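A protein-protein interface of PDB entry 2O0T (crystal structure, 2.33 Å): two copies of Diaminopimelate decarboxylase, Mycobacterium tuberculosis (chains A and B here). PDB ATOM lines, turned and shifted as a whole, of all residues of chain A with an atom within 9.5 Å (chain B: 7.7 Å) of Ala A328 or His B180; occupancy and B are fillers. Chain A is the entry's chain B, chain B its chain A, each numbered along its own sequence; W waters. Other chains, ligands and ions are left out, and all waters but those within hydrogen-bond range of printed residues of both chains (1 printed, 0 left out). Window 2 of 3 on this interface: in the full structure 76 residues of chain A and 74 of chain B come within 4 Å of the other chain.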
ATOM      1  N   ASP A 323     -21.641  24.130 -19.330  1.00  0.00           N
ATOM      2  CA  ASP A 323     -20.877  23.286 -18.453  1.00  0.00           C
ATOM      3  C   ASP A 323     -20.263  24.043 -17.269  1.00  0.00           C
ATOM      4  O   ASP A 323     -19.477  25.014 -17.459  1.00  0.00           O
ATOM      5  CB  ASP A 323     -19.831  22.476 -19.234  1.00  0.00           C
ATOM      6  CG  ASP A 323     -19.463  21.156 -18.514  1.00  0.00           C
ATOM      7  OD1 ASP A 323     -18.218  20.913 -18.469  1.00  0.00           O
ATOM      8  OD2 ASP A 323     -20.396  20.371 -18.024  1.00  0.00           O
ATOM      9  N   VAL A 324     -20.660  23.593 -16.070  1.00  0.00           N
ATOM     10  CA  VAL A 324     -20.321  24.244 -14.800  1.00  0.00           C
ATOM     11  C   VAL A 324     -19.335  23.408 -13.983  1.00  0.00           C
ATOM     12  O   VAL A 324     -19.631  22.251 -13.675  1.00  0.00           O
ATOM     13  CB  VAL A 324     -21.591  24.490 -13.957  1.00  0.00           C
ATOM     14  CG1 VAL A 324     -21.249  25.073 -12.548  1.00  0.00           C
ATOM     15  CG2 VAL A 324     -22.552  25.452 -14.719  1.00  0.00           C
ATOM     16  N   ASP A 325     -18.166  23.976 -13.688  1.00  0.00           N
ATOM     17  CA  ASP A 325     -17.120  23.373 -12.820  1.00  0.00           C
ATOM     18  C   ASP A 325     -17.663  23.190 -11.394  1.00  0.00           C
ATOM     19  O   ASP A 325     -18.153  24.153 -10.794  1.00  0.00           O
ATOM     20  CB  ASP A 325     -15.954  24.373 -12.747  1.00  0.00           C
ATOM     21  CG  ASP A 325     -16.464  25.810 -12.289  1.00  0.00           C
ATOM     22  OD1 ASP A 325     -17.390  26.396 -12.992  1.00  0.00           O
ATOM     23  OD2 ASP A 325     -15.994  26.309 -11.213  1.00  0.00           O
ATOM     24  N   VAL A 326     -17.639  21.970 -10.850  1.00  0.00           N
ATOM     25  CA  VAL A 326     -18.167  21.807  -9.495  1.00  0.00           C
ATOM     26  C   VAL A 326     -17.106  21.407  -8.504  1.00  0.00           C
ATOM     27  O   VAL A 326     -17.325  21.446  -7.312  1.00  0.00           O
ATOM     28  CB  VAL A 326     -19.502  20.940  -9.352  1.00  0.00           C
ATOM     29  CG1 VAL A 326     -20.614  21.447 -10.321  1.00  0.00           C
ATOM     30  CG2 VAL A 326     -19.238  19.475  -9.520  1.00  0.00           C
ATOM     31  N   SER A 327     -15.944  21.026  -9.004  1.00  0.00           N
ATOM     32  CA  SER A 327     -14.794  20.803  -8.171  1.00  0.00           C
ATOM     33  C   SER A 327     -13.630  20.917  -9.109  1.00  0.00           C
ATOM     34  O   SER A 327     -13.818  21.298 -10.229  1.00  0.00           O
ATOM     35  CB  SER A 327     -14.898  19.471  -7.429  1.00  0.00           C
ATOM     36  OG  SER A 327     -15.061  18.403  -8.326  1.00  0.00           O
ATOM     37  N   ALA A 328     -12.416  20.670  -8.641  1.00  0.00           N
ATOM     38  CA  ALA A 328     -11.206  20.779  -9.484  1.00  0.00           C
ATOM     39  C   ALA A 328     -11.171  19.776 -10.645  1.00  0.00           C
ATOM     40  O   ALA A 328     -10.389  19.941 -11.581  1.00  0.00           O
ATOM     41  CB  ALA A 328      -9.939  20.601  -8.631  1.00  0.00           C
ATOM     42  N   THR A 329     -11.987  18.735 -10.536  1.00  0.00           N
ATOM     43  CA  THR A 329     -12.018  17.617 -11.447  1.00  0.00           C
ATOM     44  C   THR A 329     -13.388  17.358 -12.072  1.00  0.00           C
ATOM     45  O   THR A 329     -13.461  16.807 -13.168  1.00  0.00           O
ATOM     46  CB  THR A 329     -11.569  16.256 -10.721  1.00  0.00           C
ATOM     47  OG1 THR A 329     -12.402  15.982  -9.564  1.00  0.00           O
ATOM     48  CG2 THR A 329     -10.113  16.283 -10.292  1.00  0.00           C
ATOM     49  N   ALA A 330     -14.460  17.735 -11.400  1.00  0.00           N
ATOM     50  CA  ALA A 330     -15.808  17.507 -11.917  1.00  0.00           C
ATOM     51  C   ALA A 330     -16.640  18.721 -12.378  1.00  0.00           C
ATOM     52  O   ALA A 330     -16.370  19.864 -12.014  1.00  0.00           O
ATOM     53  CB  ALA A 330     -16.641  16.640 -10.914  1.00  0.00           C
ATOM     54  N   HIS A 331     -17.702  18.410 -13.131  1.00  0.00           N
ATOM     55  CA  HIS A 331     -18.470  19.378 -13.904  1.00  0.00           C
ATOM     56  C   HIS A 331     -19.874  18.908 -13.906  1.00  0.00           C
ATOM     57  O   HIS A 331     -20.130  17.713 -13.751  1.00  0.00           O
ATOM     58  CB  HIS A 331     -17.877  19.385 -15.308  1.00  0.00           C
ATOM     59  CG  HIS A 331     -16.406  19.132 -15.272  1.00  0.00           C
ATOM     60  ND1 HIS A 331     -15.504  20.136 -15.005  1.00  0.00           N
ATOM     61  CD2 HIS A 331     -15.691  17.978 -15.325  1.00  0.00           C
ATOM     62  CE1 HIS A 331     -14.284  19.615 -14.943  1.00  0.00           C
ATOM     63  NE2 HIS A 331     -14.367  18.308 -15.145  1.00  0.00           N
ATOM     64  N   ARG A 332     -20.799  19.829 -14.050  1.00  0.00           N
ATOM     65  CA  ARG A 332     -22.205  19.453 -14.152  1.00  0.00           C
ATOM     66  C   ARG A 332     -22.785  20.239 -15.346  1.00  0.00           C
ATOM     67  O   ARG A 332     -22.473  21.394 -15.541  1.00  0.00           O
ATOM     68  CB  ARG A 332     -22.941  19.702 -12.809  1.00  0.00           C
ATOM     69  CG  ARG A 332     -24.461  19.372 -12.782  1.00  0.00           C
ATOM     70  CD  ARG A 332     -25.199  19.772 -11.471  1.00  0.00           C
ATOM     71  NE  ARG A 332     -24.410  19.809 -10.227  1.00  0.00           N
ATOM     72  CZ  ARG A 332     -23.889  18.753  -9.604  1.00  0.00           C
ATOM     73  NH1 ARG A 332     -24.005  17.541 -10.134  1.00  0.00           N
ATOM     74  NH2 ARG A 332     -23.181  18.913  -8.487  1.00  0.00           N
ATOM     75  N   TYR A 334     -25.432  22.173 -17.179  1.00  0.00           N
ATOM     76  CA  TYR A 334     -26.676  22.898 -16.949  1.00  0.00           C
ATOM     77  C   TYR A 334     -27.416  23.087 -18.272  1.00  0.00           C
ATOM     78  O   TYR A 334     -26.903  23.690 -19.269  1.00  0.00           O
ATOM     79  CB  TYR A 334     -26.431  24.232 -16.268  1.00  0.00           C
ATOM     80  CG  TYR A 334     -26.258  24.102 -14.789  1.00  0.00           C
ATOM     81  CD1 TYR A 334     -25.085  23.549 -14.239  1.00  0.00           C
ATOM     82  CD2 TYR A 334     -27.281  24.494 -13.921  1.00  0.00           C
ATOM     83  CE1 TYR A 334     -24.934  23.422 -12.871  1.00  0.00           C
ATOM     84  CE2 TYR A 334     -27.135  24.365 -12.538  1.00  0.00           C
ATOM     85  CZ  TYR A 334     -25.973  23.829 -12.015  1.00  0.00           C
ATOM     86  OH  TYR A 334     -25.842  23.686 -10.632  1.00  0.00           O
ATOM     87  N   THR B 165     -19.802  34.692 -11.915  1.00  0.00           N
ATOM     88  CA  THR B 165     -19.968  33.827 -10.760  1.00  0.00           C
ATOM     89  C   THR B 165     -18.645  33.932  -9.978  1.00  0.00           C
ATOM     90  O   THR B 165     -17.593  33.590 -10.523  1.00  0.00           O
ATOM     91  CB  THR B 165     -20.264  32.427 -11.280  1.00  0.00           C
ATOM     92  OG1 THR B 165     -21.628  32.114 -11.003  1.00  0.00           O
ATOM     93  CG2 THR B 165     -19.430  31.412 -10.666  1.00  0.00           C
ATOM     94  N   VAL B 166     -18.680  34.449  -8.741  1.00  0.00           N
ATOM     95  CA  VAL B 166     -17.435  34.668  -7.989  1.00  0.00           C
ATOM     96  C   VAL B 166     -17.340  33.843  -6.691  1.00  0.00           C
ATOM     97  O   VAL B 166     -16.473  34.066  -5.849  1.00  0.00           O
ATOM     98  CB  VAL B 166     -17.154  36.177  -7.741  1.00  0.00           C
ATOM     99  CG1 VAL B 166     -17.151  36.952  -9.071  1.00  0.00           C
ATOM    100  CG2 VAL B 166     -18.186  36.810  -6.748  1.00  0.00           C
ATOM    101  N   GLY B 167     -18.244  32.891  -6.531  1.00  0.00           N
ATOM    102  CA  GLY B 167     -18.159  31.984  -5.391  1.00  0.00           C
ATOM    103  C   GLY B 167     -18.516  32.557  -4.035  1.00  0.00           C
ATOM    104  O   GLY B 167     -18.045  32.075  -3.013  1.00  0.00           O
ATOM    105  N   SER B 177     -17.950  31.372   1.015  1.00  0.00           N
ATOM    106  CA  SER B 177     -17.169  31.397  -0.203  1.00  0.00           C
ATOM    107  C   SER B 177     -16.842  29.958  -0.654  1.00  0.00           C
ATOM    108  O   SER B 177     -16.387  29.134   0.131  1.00  0.00           O
ATOM    109  CB  SER B 177     -15.947  32.287  -0.032  1.00  0.00           C
ATOM    110  OG  SER B 177     -14.887  31.924  -0.871  1.00  0.00           O
ATOM    111  N   THR B 178     -17.128  29.659  -1.922  1.00  0.00           N
ATOM    112  CA  THR B 178     -16.801  28.346  -2.500  1.00  0.00           C
ATOM    113  C   THR B 178     -15.777  28.449  -3.607  1.00  0.00           C
ATOM    114  O   THR B 178     -15.589  29.504  -4.245  1.00  0.00           O
ATOM    115  CB  THR B 178     -18.039  27.573  -3.019  1.00  0.00           C
ATOM    116  OG1 THR B 178     -18.938  28.465  -3.724  1.00  0.00           O
ATOM    117  CG2 THR B 178     -18.789  26.961  -1.847  1.00  0.00           C
ATOM    118  N   ALA B 179     -15.113  27.327  -3.838  1.00  0.00           N
ATOM    119  CA  ALA B 179     -14.181  27.233  -4.927  1.00  0.00           C
ATOM    120  C   ALA B 179     -14.925  27.175  -6.270  1.00  0.00           C
ATOM    121  O   ALA B 179     -14.423  27.663  -7.273  1.00  0.00           O
ATOM    122  CB  ALA B 179     -13.251  25.993  -4.724  1.00  0.00           C
ATOM    123  N   HIS B 180     -16.117  26.585  -6.270  1.00  0.00           N
ATOM    124  CA  HIS B 180     -16.895  26.366  -7.486  1.00  0.00           C
ATOM    125  C   HIS B 180     -18.355  26.543  -7.110  1.00  0.00           C
ATOM    126  O   HIS B 180     -18.907  25.726  -6.403  1.00  0.00           O
ATOM    127  CB  HIS B 180     -16.648  24.937  -8.035  1.00  0.00           C
ATOM    128  CG  HIS B 180     -15.205  24.623  -8.298  1.00  0.00           C
ATOM    129  ND1 HIS B 180     -14.530  25.081  -9.410  1.00  0.00           N
ATOM    130  CD2 HIS B 180     -14.301  23.921  -7.577  1.00  0.00           C
ATOM    131  CE1 HIS B 180     -13.272  24.687  -9.354  1.00  0.00           C
ATOM    132  NE2 HIS B 180     -13.107  23.981  -8.251  1.00  0.00           N
ATOM    133  N   GLU B 181     -18.970  27.625  -7.563  1.00  0.00           N
ATOM    134  CA  GLU B 181     -20.378  27.864  -7.345  1.00  0.00           C
ATOM    135  C   GLU B 181     -21.088  26.918  -8.330  1.00  0.00           C
ATOM    136  O   GLU B 181     -20.776  26.896  -9.527  1.00  0.00           O
ATOM    137  CB  GLU B 181     -20.702  29.343  -7.613  1.00  0.00           C
ATOM    138  CG  GLU B 181     -21.714  29.997  -6.642  1.00  0.00           C
ATOM    139  CD  GLU B 181     -22.075  31.453  -7.043  1.00  0.00           C
ATOM    140  OE1 GLU B 181     -21.164  32.221  -7.423  1.00  0.00           O
ATOM    141  OE2 GLU B 181     -23.276  31.836  -6.980  1.00  0.00           O
ATOM    142  N   ASP B 182     -22.035  26.136  -7.827  1.00  0.00           N
ATOM    143  CA  ASP B 182     -22.657  25.077  -8.601  1.00  0.00           C
ATOM    144  C   ASP B 182     -24.095  25.600  -8.857  1.00  0.00           C
ATOM    145  O   ASP B 182     -25.025  25.291  -8.167  1.00  0.00           O
ATOM    146  CB  ASP B 182     -22.571  23.850  -7.719  1.00  0.00           C
ATOM    147  CG  ASP B 182     -23.185  22.624  -8.302  1.00  0.00           C
ATOM    148  OD1 ASP B 182     -23.111  21.609  -7.586  1.00  0.00           O
ATOM    149  OD2 ASP B 182     -23.725  22.637  -9.417  1.00  0.00           O
ATOM    150  N   GLN B 183     -24.253  26.458  -9.848  1.00  0.00           N
ATOM    151  CA  GLN B 183     -25.592  26.986 -10.173  1.00  0.00           C
ATOM    152  C   GLN B 183     -25.637  27.512 -11.604  1.00  0.00           C
ATOM    153  O   GLN B 183     -24.631  27.484 -12.301  1.00  0.00           O
ATOM    154  CB  GLN B 183     -26.076  28.011  -9.124  1.00  0.00           C
ATOM    155  CG  GLN B 183     -25.071  29.131  -8.817  1.00  0.00           C
ATOM    156  CD  GLN B 183     -25.058  30.199  -9.912  1.00  0.00           C
ATOM    157  OE1 GLN B 183     -26.081  30.850 -10.158  1.00  0.00           O
ATOM    158  NE2 GLN B 183     -23.911  30.377 -10.575  1.00  0.00           N
ATOM    159  N   SER B 188     -17.633  31.712 -14.664  1.00  0.00           N
ATOM    160  CA  SER B 188     -16.667  31.632 -13.622  1.00  0.00           C
ATOM    161  C   SER B 188     -15.424  32.452 -13.930  1.00  0.00           C
ATOM    162  O   SER B 188     -14.718  32.241 -14.950  1.00  0.00           O
ATOM    163  CB  SER B 188     -16.312  30.169 -13.367  1.00  0.00           C
ATOM    164  OG  SER B 188     -15.222  30.082 -12.475  1.00  0.00           O
ATOM    165  N   ALA B 190     -12.819  32.471 -11.831  1.00  0.00           N
ATOM    166  CA  ALA B 190     -11.794  31.480 -11.495  1.00  0.00           C
ATOM    167  C   ALA B 190     -11.371  30.506 -12.627  1.00  0.00           C
ATOM    168  O   ALA B 190     -10.225  30.210 -12.766  1.00  0.00           O
ATOM    169  CB  ALA B 190     -12.233  30.691 -10.231  1.00  0.00           C
ATOM    170  N   SER B 191     -12.324  30.000 -13.404  1.00  0.00           N
ATOM    171  CA  SER B 191     -12.044  28.976 -14.437  1.00  0.00           C
ATOM    172  C   SER B 191     -11.487  29.559 -15.733  1.00  0.00           C
ATOM    173  O   SER B 191     -11.012  28.810 -16.608  1.00  0.00           O
ATOM    174  CB  SER B 191     -13.329  28.218 -14.772  1.00  0.00           C
ATOM    175  OG  SER B 191     -14.168  29.011 -15.582  1.00  0.00           O
HETATM  176  O   HOH W   1     -27.873  24.885  -8.810  1.00  0.00           O
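A ring nitrogen (ND1) of His B180 is in hydrogen-bond range of the side-chain carboxylate (OD2) of Asp A325.
A ring nitrogen (NE2) of His B180 lies close to the backbone carbonyl oxygen (O) of Ser A327 (3.4 Å).
The backbone NH of Ala A328 is in hydrogen-bond range of a ring nitrogen (NE2) of His B180, 3.4 Å away.
The guanidinium group (NH2) of Arg A332 lies within salt-bridge range of the side-chain carboxylate (OD1) of Asp B182 (2.8 Å).
OH of Tyr A334 lies within hydrogen-bond range of OD2 of Asp B182 (2.7 Å).
The backbone NH (N) of Gln B183 lies within hydrogen-bond range of the side-chain hydroxyl (OH) of Tyr A334 (3.3 Å).
Printed residues of chain A that touch a printed residue of chain B: Val A324, Asp A325, Val A326, Ser A327, Ala A328, Arg A332 and Tyr A334.
Along chain A the printed residues that touch a printed residue of chain B span positions 324 to 334.
Of the 13 printed residues of chain B, 5 touch a printed residue of chain A.
Hydrophobic or aromatic side chains of chain B that line the printed part of chain A: His B180.
Among the printed residues, 11 pairs touch across the chains.
His B180 touches four residues of chain A.
Of chain B, only His B180 (3.2 Å) comes within 4 Å of Ser A327.
Ala B179 touches none of the printed residues of chain A.
Printed residues of chain B within 4 Å of Arg A332: Asp B182.
Of the printed residues of chain B, Val A324 touches Glu B181 and Gln B183.
Val B166 touches none of the printed residues of chain A.
The nearest printed residue of chain A that does not touch Gln B183 is Val A326 (6.2 Å).
No position is printed for both chains.
The side-chain amide nitrogen (NE2) of Gln B183 lies within hydrogen-bond range of the side-chain hydroxyl (OG1) of Thr B165 (2.9 Å).
OE1 of Glu B181 lies within hydrogen-bond range of N of Gly B167 (3.1 Å).
OG of Ser B188 lies close to N of Ala B190, at 3.4 Å.
The side-chain hydroxyl (OG) of Ser B188 sits at hydrogen-bond distance from the backbone NH (N) of Ser B191 (3.0 Å).
The backbone NH (N) of Arg A332 sits at hydrogen-bond distance from the backbone carbonyl oxygen (O) of Val A324 (2.7 Å).
OG of Ser A327 is in hydrogen-bond range of N of Ala A330 (3.2 Å).
Among the printed residues, merely in contact across the chains: Val A326 with Asp B182 (3.5 Å), Val A324 with Glu B181 (3.6 Å), Val A326 with His B180 (3.6 Å), Val A324 with Gln B183 (3.8 Å) and Asp A325 with Ser B188 (3.9 Å).
Water W1 bridges the backbone carbonyl oxygen of Asp B182 and the side-chain hydroxyl of Tyr A334.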
